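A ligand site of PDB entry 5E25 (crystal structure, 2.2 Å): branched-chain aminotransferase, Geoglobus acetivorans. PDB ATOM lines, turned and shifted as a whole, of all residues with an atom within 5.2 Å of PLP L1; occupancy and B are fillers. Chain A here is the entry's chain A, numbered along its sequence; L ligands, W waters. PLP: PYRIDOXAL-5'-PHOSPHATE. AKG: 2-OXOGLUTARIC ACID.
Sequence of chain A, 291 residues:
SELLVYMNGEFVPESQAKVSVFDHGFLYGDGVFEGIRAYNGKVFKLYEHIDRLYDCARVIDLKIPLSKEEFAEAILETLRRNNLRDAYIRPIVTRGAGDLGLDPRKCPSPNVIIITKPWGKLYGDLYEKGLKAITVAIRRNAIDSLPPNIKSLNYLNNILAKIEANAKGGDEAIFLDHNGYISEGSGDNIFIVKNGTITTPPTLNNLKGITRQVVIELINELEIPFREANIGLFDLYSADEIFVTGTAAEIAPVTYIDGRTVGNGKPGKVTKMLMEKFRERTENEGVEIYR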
ATOM      1  N   PHE A  33     -15.971  -6.112 -24.527  1.00  0.00           N
ATOM      2  CA  PHE A  33     -15.662  -5.875 -25.927  1.00  0.00           C
ATOM      3  C   PHE A  33     -15.966  -7.105 -26.735  1.00  0.00           C
ATOM      4  O   PHE A  33     -16.333  -8.148 -26.160  1.00  0.00           O
ATOM      5  CB  PHE A  33     -14.202  -5.432 -26.198  1.00  0.00           C
ATOM      6  CG  PHE A  33     -13.187  -6.545 -26.096  1.00  0.00           C
ATOM      7  CD1 PHE A  33     -12.651  -6.894 -24.830  1.00  0.00           C
ATOM      8  CD2 PHE A  33     -12.737  -7.233 -27.236  1.00  0.00           C
ATOM      9  CE1 PHE A  33     -11.666  -7.904 -24.726  1.00  0.00           C
ATOM     10  CE2 PHE A  33     -11.759  -8.241 -27.137  1.00  0.00           C
ATOM     11  CZ  PHE A  33     -11.224  -8.566 -25.879  1.00  0.00           C
ATOM     12  N   GLY A  35     -15.076  -8.966 -30.898  1.00  0.00           N
ATOM     13  CA  GLY A  35     -14.220  -9.037 -32.071  1.00  0.00           C
ATOM     14  C   GLY A  35     -15.041  -9.727 -33.149  1.00  0.00           C
ATOM     15  O   GLY A  35     -15.542 -10.837 -32.905  1.00  0.00           O
ATOM     16  N   HIS A  49     -22.201 -12.447 -31.888  1.00  0.00           N
ATOM     17  CA  HIS A  49     -21.245 -11.622 -31.220  1.00  0.00           C
ATOM     18  C   HIS A  49     -21.939 -10.583 -30.347  1.00  0.00           C
ATOM     19  O   HIS A  49     -21.545 -10.321 -29.170  1.00  0.00           O
ATOM     20  CB  HIS A  49     -20.295 -11.046 -32.246  1.00  0.00           C
ATOM     21  CG  HIS A  49     -19.249 -12.028 -32.683  1.00  0.00           C
ATOM     22  ND1 HIS A  49     -18.101 -12.276 -31.949  1.00  0.00           N
ATOM     23  CD2 HIS A  49     -19.163 -12.824 -33.778  1.00  0.00           C
ATOM     24  CE1 HIS A  49     -17.349 -13.168 -32.581  1.00  0.00           C
ATOM     25  NE2 HIS A  49     -17.958 -13.501 -33.702  1.00  0.00           N
ATOM     26  N   ARG A  52     -23.312 -12.183 -27.250  1.00  0.00           N
ATOM     27  CA  ARG A  52     -22.258 -12.423 -26.236  1.00  0.00           C
ATOM     28  C   ARG A  52     -21.890 -11.070 -25.556  1.00  0.00           C
ATOM     29  O   ARG A  52     -21.830 -10.957 -24.305  1.00  0.00           O
ATOM     30  CB  ARG A  52     -21.040 -13.159 -26.858  1.00  0.00           C
ATOM     31  CG  ARG A  52     -20.119 -13.676 -25.758  1.00  0.00           C
ATOM     32  CD  ARG A  52     -18.891 -14.381 -26.276  1.00  0.00           C
ATOM     33  NE  ARG A  52     -18.074 -13.574 -27.174  1.00  0.00           N
ATOM     34  CZ  ARG A  52     -17.254 -14.137 -28.065  1.00  0.00           C
ATOM     35  NH1 ARG A  52     -17.169 -15.480 -28.112  1.00  0.00           N
ATOM     36  NH2 ARG A  52     -16.488 -13.391 -28.861  1.00  0.00           N
ATOM     37  N   ARG A 140      -4.870 -19.438 -15.922  1.00  0.00           N
ATOM     38  CA  ARG A 140      -5.983 -18.591 -16.425  1.00  0.00           C
ATOM     39  C   ARG A 140      -6.698 -18.015 -15.232  1.00  0.00           C
ATOM     40  O   ARG A 140      -6.817 -18.713 -14.202  1.00  0.00           O
ATOM     41  CB  ARG A 140      -7.001 -19.424 -17.210  1.00  0.00           C
ATOM     42  CG  ARG A 140      -8.055 -18.578 -17.983  1.00  0.00           C
ATOM     43  CD  ARG A 140      -7.399 -18.030 -19.269  1.00  0.00           C
ATOM     44  NE  ARG A 140      -8.370 -17.367 -20.160  1.00  0.00           N
ATOM     45  CZ  ARG A 140      -8.832 -16.108 -20.045  1.00  0.00           C
ATOM     46  NH1 ARG A 140      -8.457 -15.260 -19.046  1.00  0.00           N
ATOM     47  NH2 ARG A 140      -9.741 -15.742 -20.925  1.00  0.00           N
ATOM     48  N   LYS A 151     -15.665 -11.385 -21.905  1.00  0.00           N
ATOM     49  CA  LYS A 151     -14.727 -10.711 -22.842  1.00  0.00           C
ATOM     50  C   LYS A 151     -14.683  -9.281 -22.390  1.00  0.00           C
ATOM     51  O   LYS A 151     -15.468  -8.440 -22.867  1.00  0.00           O
ATOM     52  CB  LYS A 151     -15.249 -10.761 -24.274  1.00  0.00           C
ATOM     53  CG  LYS A 151     -14.137 -10.911 -25.283  1.00  0.00           C
ATOM     54  CD  LYS A 151     -14.792 -11.430 -26.547  1.00  0.00           C
ATOM     55  CE  LYS A 151     -13.722 -11.307 -27.597  1.00  0.00           C
ATOM     56  NZ  LYS A 151     -12.685 -12.295 -27.422  1.00  0.00           N
ATOM     57  N   TYR A 155      -7.702  -7.565 -19.434  1.00  0.00           N
ATOM     58  CA  TYR A 155      -6.987  -8.592 -20.172  1.00  0.00           C
ATOM     59  C   TYR A 155      -5.524  -8.731 -19.798  1.00  0.00           C
ATOM     60  O   TYR A 155      -4.735  -9.244 -20.576  1.00  0.00           O
ATOM     61  CB  TYR A 155      -7.200  -8.427 -21.724  1.00  0.00           C
ATOM     62  CG  TYR A 155      -8.275  -9.390 -22.250  1.00  0.00           C
ATOM     63  CD1 TYR A 155      -9.474  -9.533 -21.554  1.00  0.00           C
ATOM     64  CD2 TYR A 155      -8.050 -10.191 -23.398  1.00  0.00           C
ATOM     65  CE1 TYR A 155     -10.446 -10.442 -21.981  1.00  0.00           C
ATOM     66  CE2 TYR A 155      -9.009 -11.083 -23.850  1.00  0.00           C
ATOM     67  CZ  TYR A 155     -10.207 -11.186 -23.112  1.00  0.00           C
ATOM     68  OH  TYR A 155     -11.185 -12.042 -23.471  1.00  0.00           O
ATOM     69  N   ASN A 158      -4.231 -12.284 -19.811  1.00  0.00           N
ATOM     70  CA  ASN A 158      -3.949 -12.772 -21.163  1.00  0.00           C
ATOM     71  C   ASN A 158      -2.642 -12.167 -21.629  1.00  0.00           C
ATOM     72  O   ASN A 158      -1.828 -12.870 -22.229  1.00  0.00           O
ATOM     73  CB  ASN A 158      -5.093 -12.367 -22.071  1.00  0.00           C
ATOM     74  CG  ASN A 158      -6.442 -12.790 -21.519  1.00  0.00           C
ATOM     75  OD1 ASN A 158      -7.102 -13.688 -22.083  1.00  0.00           O
ATOM     76  ND2 ASN A 158      -6.872 -12.182 -20.427  1.00  0.00           N
ATOM     77  N   GLU A 184      -6.945 -22.662 -22.703  1.00  0.00           N
ATOM     78  CA  GLU A 184      -7.028 -22.021 -24.028  1.00  0.00           C
ATOM     79  C   GLU A 184      -5.735 -21.300 -24.288  1.00  0.00           C
ATOM     80  O   GLU A 184      -4.905 -21.134 -23.376  1.00  0.00           O
ATOM     81  CB  GLU A 184      -8.203 -21.002 -24.099  1.00  0.00           C
ATOM     82  CG  GLU A 184      -8.204 -19.911 -23.044  1.00  0.00           C
ATOM     83  CD  GLU A 184      -9.268 -18.844 -23.306  1.00  0.00           C
ATOM     84  OE1 GLU A 184      -9.703 -18.735 -24.464  1.00  0.00           O
ATOM     85  OE2 GLU A 184      -9.651 -18.077 -22.390  1.00  0.00           O
ATOM     86  N   GLY A 185      -5.549 -20.855 -25.516  1.00  0.00           N
ATOM     87  CA  GLY A 185      -4.533 -19.810 -25.812  1.00  0.00           C
ATOM     88  C   GLY A 185      -4.827 -18.433 -25.189  1.00  0.00           C
ATOM     89  O   GLY A 185      -5.880 -18.223 -24.586  1.00  0.00           O
ATOM     90  N   SER A 186      -3.894 -17.479 -25.324  1.00  0.00           N
ATOM     91  CA  SER A 186      -4.080 -16.139 -24.681  1.00  0.00           C
ATOM     92  C   SER A 186      -5.271 -15.402 -25.235  1.00  0.00           C
ATOM     93  O   SER A 186      -5.858 -14.544 -24.555  1.00  0.00           O
ATOM     94  CB  SER A 186      -2.866 -15.249 -24.878  1.00  0.00           C
ATOM     95  OG  SER A 186      -2.554 -15.120 -26.267  1.00  0.00           O
ATOM     96  N   GLY A 187      -5.598 -15.690 -26.497  1.00  0.00           N
ATOM     97  CA  GLY A 187      -6.674 -15.041 -27.209  1.00  0.00           C
ATOM     98  C   GLY A 187      -7.498 -15.937 -28.127  1.00  0.00           C
ATOM     99  O   GLY A 187      -8.287 -15.426 -28.962  1.00  0.00           O
ATOM    100  N   ASP A 188      -7.328 -17.243 -27.983  1.00  0.00           N
ATOM    101  CA  ASP A 188      -8.099 -18.175 -28.818  1.00  0.00           C
ATOM    102  C   ASP A 188      -8.343 -19.527 -28.150  1.00  0.00           C
ATOM    103  O   ASP A 188      -7.610 -19.922 -27.248  1.00  0.00           O
ATOM    104  CB  ASP A 188      -7.434 -18.319 -30.196  1.00  0.00           C
ATOM    105  CG  ASP A 188      -5.963 -18.128 -30.151  1.00  0.00           C
ATOM    106  OD1 ASP A 188      -5.297 -18.631 -29.205  1.00  0.00           O
ATOM    107  OD2 ASP A 188      -5.456 -17.479 -31.082  1.00  0.00           O
ATOM    108  N   ASN A 189      -9.389 -20.224 -28.553  1.00  0.00           N
ATOM    109  CA  ASN A 189      -9.737 -21.559 -27.978  1.00  0.00           C
ATOM    110  C   ASN A 189      -8.821 -22.613 -28.489  1.00  0.00           C
ATOM    111  O   ASN A 189      -8.110 -22.362 -29.447  1.00  0.00           O
ATOM    112  CB  ASN A 189     -11.179 -21.937 -28.236  1.00  0.00           C
ATOM    113  CG  ASN A 189     -12.123 -21.056 -27.465  1.00  0.00           C
ATOM    114  OD1 ASN A 189     -12.808 -20.202 -28.053  1.00  0.00           O
ATOM    115  ND2 ASN A 189     -12.159 -21.235 -26.112  1.00  0.00           N
ATOM    116  N   LEU A 207     -13.432 -19.484 -22.629  1.00  0.00           N
ATOM    117  CA  LEU A 207     -14.295 -18.464 -23.180  1.00  0.00           C
ATOM    118  C   LEU A 207     -15.101 -19.187 -24.254  1.00  0.00           C
ATOM    119  O   LEU A 207     -14.515 -19.940 -25.072  1.00  0.00           O
ATOM    120  CB  LEU A 207     -13.463 -17.294 -23.755  1.00  0.00           C
ATOM    121  CG  LEU A 207     -14.321 -16.009 -24.079  1.00  0.00           C
ATOM    122  CD1 LEU A 207     -13.607 -14.724 -23.755  1.00  0.00           C
ATOM    123  CD2 LEU A 207     -14.860 -15.956 -25.538  1.00  0.00           C
ATOM    124  N   LYS A 208     -16.423 -18.926 -24.273  1.00  0.00           N
ATOM    125  CA  LYS A 208     -17.347 -19.532 -25.253  1.00  0.00           C
ATOM    126  C   LYS A 208     -17.164 -18.960 -26.657  1.00  0.00           C
ATOM    127  O   LYS A 208     -17.927 -18.110 -27.095  1.00  0.00           O
ATOM    128  CB  LYS A 208     -18.780 -19.360 -24.769  1.00  0.00           C
ATOM    129  CG  LYS A 208     -19.696 -20.451 -25.253  1.00  0.00           C
ATOM    130  CD  LYS A 208     -21.024 -20.386 -24.517  1.00  0.00           C
ATOM    131  CE  LYS A 208     -21.967 -21.477 -25.000  1.00  0.00           C
ATOM    132  NZ  LYS A 208     -22.311 -21.174 -26.422  1.00  0.00           N
ATOM    133  N   GLY A 209     -16.132 -19.404 -27.352  1.00  0.00           N
ATOM    134  CA  GLY A 209     -15.725 -18.859 -28.665  1.00  0.00           C
ATOM    135  C   GLY A 209     -16.802 -19.014 -29.723  1.00  0.00           C
ATOM    136  O   GLY A 209     -17.399 -20.080 -29.868  1.00  0.00           O
ATOM    137  N   ILE A 210     -17.053 -17.958 -30.486  1.00  0.00           N
ATOM    138  CA  ILE A 210     -17.965 -18.091 -31.650  1.00  0.00           C
ATOM    139  C   ILE A 210     -17.277 -18.907 -32.744  1.00  0.00           C
ATOM    140  O   ILE A 210     -17.890 -19.789 -33.358  1.00  0.00           O
ATOM    141  CB  ILE A 210     -18.579 -16.716 -32.025  1.00  0.00           C
ATOM    142  CG1 ILE A 210     -19.692 -16.438 -30.992  1.00  0.00           C
ATOM    143  CG2 ILE A 210     -19.117 -16.720 -33.471  1.00  0.00           C
ATOM    144  CD1 ILE A 210     -19.906 -14.978 -30.606  1.00  0.00           C
ATOM    145  N   THR A 211     -15.962 -18.744 -32.885  1.00  0.00           N
ATOM    146  CA  THR A 211     -15.276 -19.576 -33.888  1.00  0.00           C
ATOM    147  C   THR A 211     -15.296 -21.076 -33.489  1.00  0.00           C
ATOM    148  O   THR A 211     -15.473 -21.972 -34.328  1.00  0.00           O
ATOM    149  CB  THR A 211     -13.835 -19.152 -34.096  1.00  0.00           C
ATOM    150  OG1 THR A 211     -13.785 -17.736 -34.181  1.00  0.00           O
ATOM    151  CG2 THR A 211     -13.243 -19.794 -35.385  1.00  0.00           C
ATOM    152  N   ARG A 212     -15.044 -21.320 -32.193  1.00  0.00           N
ATOM    153  CA  ARG A 212     -15.052 -22.644 -31.616  1.00  0.00           C
ATOM    154  C   ARG A 212     -16.448 -23.229 -31.879  1.00  0.00           C
ATOM    155  O   ARG A 212     -16.538 -24.345 -32.264  1.00  0.00           O
ATOM    156  CB  ARG A 212     -14.719 -22.535 -30.106  1.00  0.00           C
ATOM    157  CG  ARG A 212     -15.129 -23.718 -29.275  1.00  0.00           C
ATOM    158  CD  ARG A 212     -14.848 -23.452 -27.766  1.00  0.00           C
ATOM    159  NE  ARG A 212     -15.004 -24.655 -26.968  1.00  0.00           N
ATOM    160  CZ  ARG A 212     -16.156 -25.332 -26.717  1.00  0.00           C
ATOM    161  NH1 ARG A 212     -17.373 -24.943 -27.190  1.00  0.00           N
ATOM    162  NH2 ARG A 212     -16.068 -26.415 -25.932  1.00  0.00           N
ATOM    163  N   THR A 245      -8.482 -21.481 -32.261  1.00  0.00           N
ATOM    164  CA  THR A 245      -9.537 -20.757 -32.944  1.00  0.00           C
ATOM    165  C   THR A 245      -9.907 -19.458 -32.304  1.00  0.00           C
ATOM    166  O   THR A 245     -10.053 -19.386 -31.092  1.00  0.00           O
ATOM    167  CB  THR A 245     -10.865 -21.587 -33.048  1.00  0.00           C
ATOM    168  OG1 THR A 245     -11.552 -21.630 -31.778  1.00  0.00           O
ATOM    169  CG2 THR A 245     -10.587 -22.962 -33.544  1.00  0.00           C
ATOM    170  N   GLY A 246     -10.195 -18.462 -33.150  1.00  0.00           N
ATOM    171  CA  GLY A 246     -10.786 -17.182 -32.727  1.00  0.00           C
ATOM    172  C   GLY A 246     -11.131 -16.288 -33.926  1.00  0.00           C
ATOM    173  O   GLY A 246     -10.722 -16.591 -35.058  1.00  0.00           O
ATOM    174  N   THR A 247     -11.855 -15.189 -33.699  1.00  0.00           N
ATOM    175  CA  THR A 247     -12.266 -14.302 -34.808  1.00  0.00           C
ATOM    176  C   THR A 247     -11.063 -13.785 -35.569  1.00  0.00           C
ATOM    177  O   THR A 247     -10.999 -13.943 -36.773  1.00  0.00           O
ATOM    178  CB  THR A 247     -13.209 -13.180 -34.386  1.00  0.00           C
ATOM    179  OG1 THR A 247     -14.376 -13.785 -33.816  1.00  0.00           O
ATOM    180  CG2 THR A 247     -13.612 -12.280 -35.640  1.00  0.00           C
ATOM    181  N   ALA A 248     -10.070 -13.286 -34.853  1.00  0.00           N
ATOM    182  CA  ALA A 248      -8.934 -12.680 -35.495  1.00  0.00           C
ATOM    183  C   ALA A 248      -8.078 -13.763 -36.116  1.00  0.00           C
ATOM    184  O   ALA A 248      -7.679 -13.658 -37.287  1.00  0.00           O
ATOM    185  CB  ALA A 248      -8.146 -11.865 -34.482  1.00  0.00           C
HETATM  186  N1  PLP L   1     -10.405 -16.604 -26.063  1.00  0.00           N
HETATM  187  C2  PLP L   1     -10.325 -15.363 -25.537  1.00  0.00           C
HETATM  188  C2A PLP L   1      -9.572 -15.135 -24.241  1.00  0.00           C
HETATM  189  C3  PLP L   1     -10.992 -14.226 -26.233  1.00  0.00           C
HETATM  190  O3  PLP L   1     -10.934 -12.973 -25.709  1.00  0.00           O
HETATM  191  C4  PLP L   1     -11.715 -14.522 -27.507  1.00  0.00           C
HETATM  192  C4A PLP L   1     -12.469 -13.423 -28.284  1.00  0.00           C
HETATM  193  C5  PLP L   1     -11.647 -15.937 -27.975  1.00  0.00           C
HETATM  194  C6  PLP L   1     -11.015 -16.923 -27.194  1.00  0.00           C
HETATM  195  C5A PLP L   1     -12.269 -16.407 -29.262  1.00  0.00           C
HETATM  196  O4P PLP L   1     -13.625 -16.008 -29.356  1.00  0.00           O
HETATM  197  P   PLP L   1     -14.293 -15.941 -30.833  1.00  0.00           P
HETATM  198  O1P PLP L   1     -13.434 -14.892 -31.490  1.00  0.00           O
HETATM  199  O2P PLP L   1     -13.997 -17.211 -31.535  1.00  0.00           O
HETATM  200  O3P PLP L   1     -15.694 -15.631 -30.390  1.00  0.00           O
HETATM  201  C1  AKG L   2     -10.726 -11.895 -31.517  1.00  0.00           C
HETATM  202  O1  AKG L   2     -11.248 -11.011 -32.237  1.00  0.00           O
HETATM  203  O2  AKG L   2     -10.497 -13.070 -31.913  1.00  0.00           O
HETATM  204  C2  AKG L   2     -10.391 -11.472 -30.148  1.00  0.00           C
HETATM  205  O5  AKG L   2     -10.937 -10.439 -29.772  1.00  0.00           O
HETATM  206  C3  AKG L   2      -9.384 -12.241 -29.284  1.00  0.00           C
HETATM  207  C4  AKG L   2      -8.746 -11.443 -28.150  1.00  0.00           C
HETATM  208  C5  AKG L   2      -8.015 -10.137 -28.553  1.00  0.00           C
HETATM  209  O3  AKG L   2      -7.905  -9.291 -27.652  1.00  0.00           O
HETATM  210  O4  AKG L   2      -7.546  -9.912 -29.706  1.00  0.00           O
HETATM  211  O   HOH W   1     -14.292 -12.270 -30.811  1.00  0.00           O
HETATM  212  O   HOH W   2     -13.166 -19.695 -30.840  1.00  0.00           O
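A carbon (C4A) of PLP L1 is bonded to the side-chain amino group of Lys 151, 1.4 Å away.
An oxygen (O1P) of PLP L1 sits at hydrogen-bond distance from the side-chain hydroxyl (OG1) of Thr 247 (2.7 Å).
The side-chain hydroxyl of Thr 211 lies within hydrogen-bond range of an oxygen (O2P) of PLP L1.
A nitrogen (N1) of PLP L1 sits at hydrogen-bond distance from the side-chain carboxylate (OE1) of Glu 184 (2.8 Å).
N of Ala 248 is in hydrogen-bond range of O2 of AKG L2 (3.0 Å).
N of Thr 247 sits at hydrogen-bond distance from O2 of AKG L2 (3.1 Å).
The side-chain hydroxyl (OH) of Tyr 155 lies within hydrogen-bond range of an oxygen (O3) of PLP L1, at 2.4 Å.
N of Ile 210 sits at hydrogen-bond distance from O3P of PLP L1 (2.7 Å).
N of Thr 247 is in hydrogen-bond range of O1P of PLP L1.
An oxygen (O3P) of PLP L1 is in salt-bridge range of the guanidinium group (NH1) of Arg 52.
The side-chain amino group (NZ) of Lys 151 sits at hydrogen-bond distance from an oxygen (O5) of AKG L2 (3.5 Å).
The backbone NH (N) of Thr 211 lies within hydrogen-bond range of an oxygen (O2P) of PLP L1, at 2.8 Å.
The backbone NH (N) of Phe 33 lies within hydrogen-bond range of the backbone carbonyl oxygen (O) of Lys 151, at 2.9 Å.
The side-chain amide oxygen (OD1) of Asn 189 lies close to the backbone NH (N) of Gly 209, 3.5 Å away.
OG1 of Thr 211 lies within hydrogen-bond range of N of Thr 247, at 3.2 Å.
NH1 of Arg 52 lies within hydrogen-bond range of O of Lys 208, 2.9 Å away.
The backbone carbonyl oxygen of Leu 207 is in hydrogen-bond range of the side-chain amide nitrogen of Asn 189 (2.9 Å).
The backbone NH of Asn 189 lies within hydrogen-bond range of the backbone carbonyl oxygen of Thr 245 (2.8 Å).
OG1 of Thr 211 sits close to O of Gly 246 (3.4 Å).
OG1 of Thr 247 is in hydrogen-bond range of O of Gly 35 (3.3 Å).
Merely in contact with PLP L1: Arg 140 (3.4 Å), Gly 246 (3.4 Å), Gly 187 (3.5 Å), Asp 188 (3.6 Å), Asn 158 (3.6 Å), Gly 209 (3.6 Å), Leu 207 (3.6 Å), His 49 (3.7 Å), Ser 186 (3.8 Å) and Asn 189 (3.8 Å).
17 residues have an atom within 4 Å of PLP L1: His 49, Arg 52, Arg 140, Lys 151, Tyr 155, Asn 158, Glu 184, Ser 186, Gly 187, Asp 188, Asn 189, Leu 207, Gly 209, Ile 210, Thr 211, Gly 246 and Thr 247.
Water W2 lies within hydrogen-bond range of OG1 of Thr 245 (2.7 Å), O2P of PLP L1 (2.7 Å), N of Arg 212 (2.8 Å) and OD1 of Asn 189 (2.9 Å).
Water W1 lies within hydrogen-bond range of O of Gly 35 (2.8 Å), O1P of PLP L1 (2.8 Å), NH2 of Arg 52 (3.1 Å) and OG1 of Thr 247 (3.4 Å).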
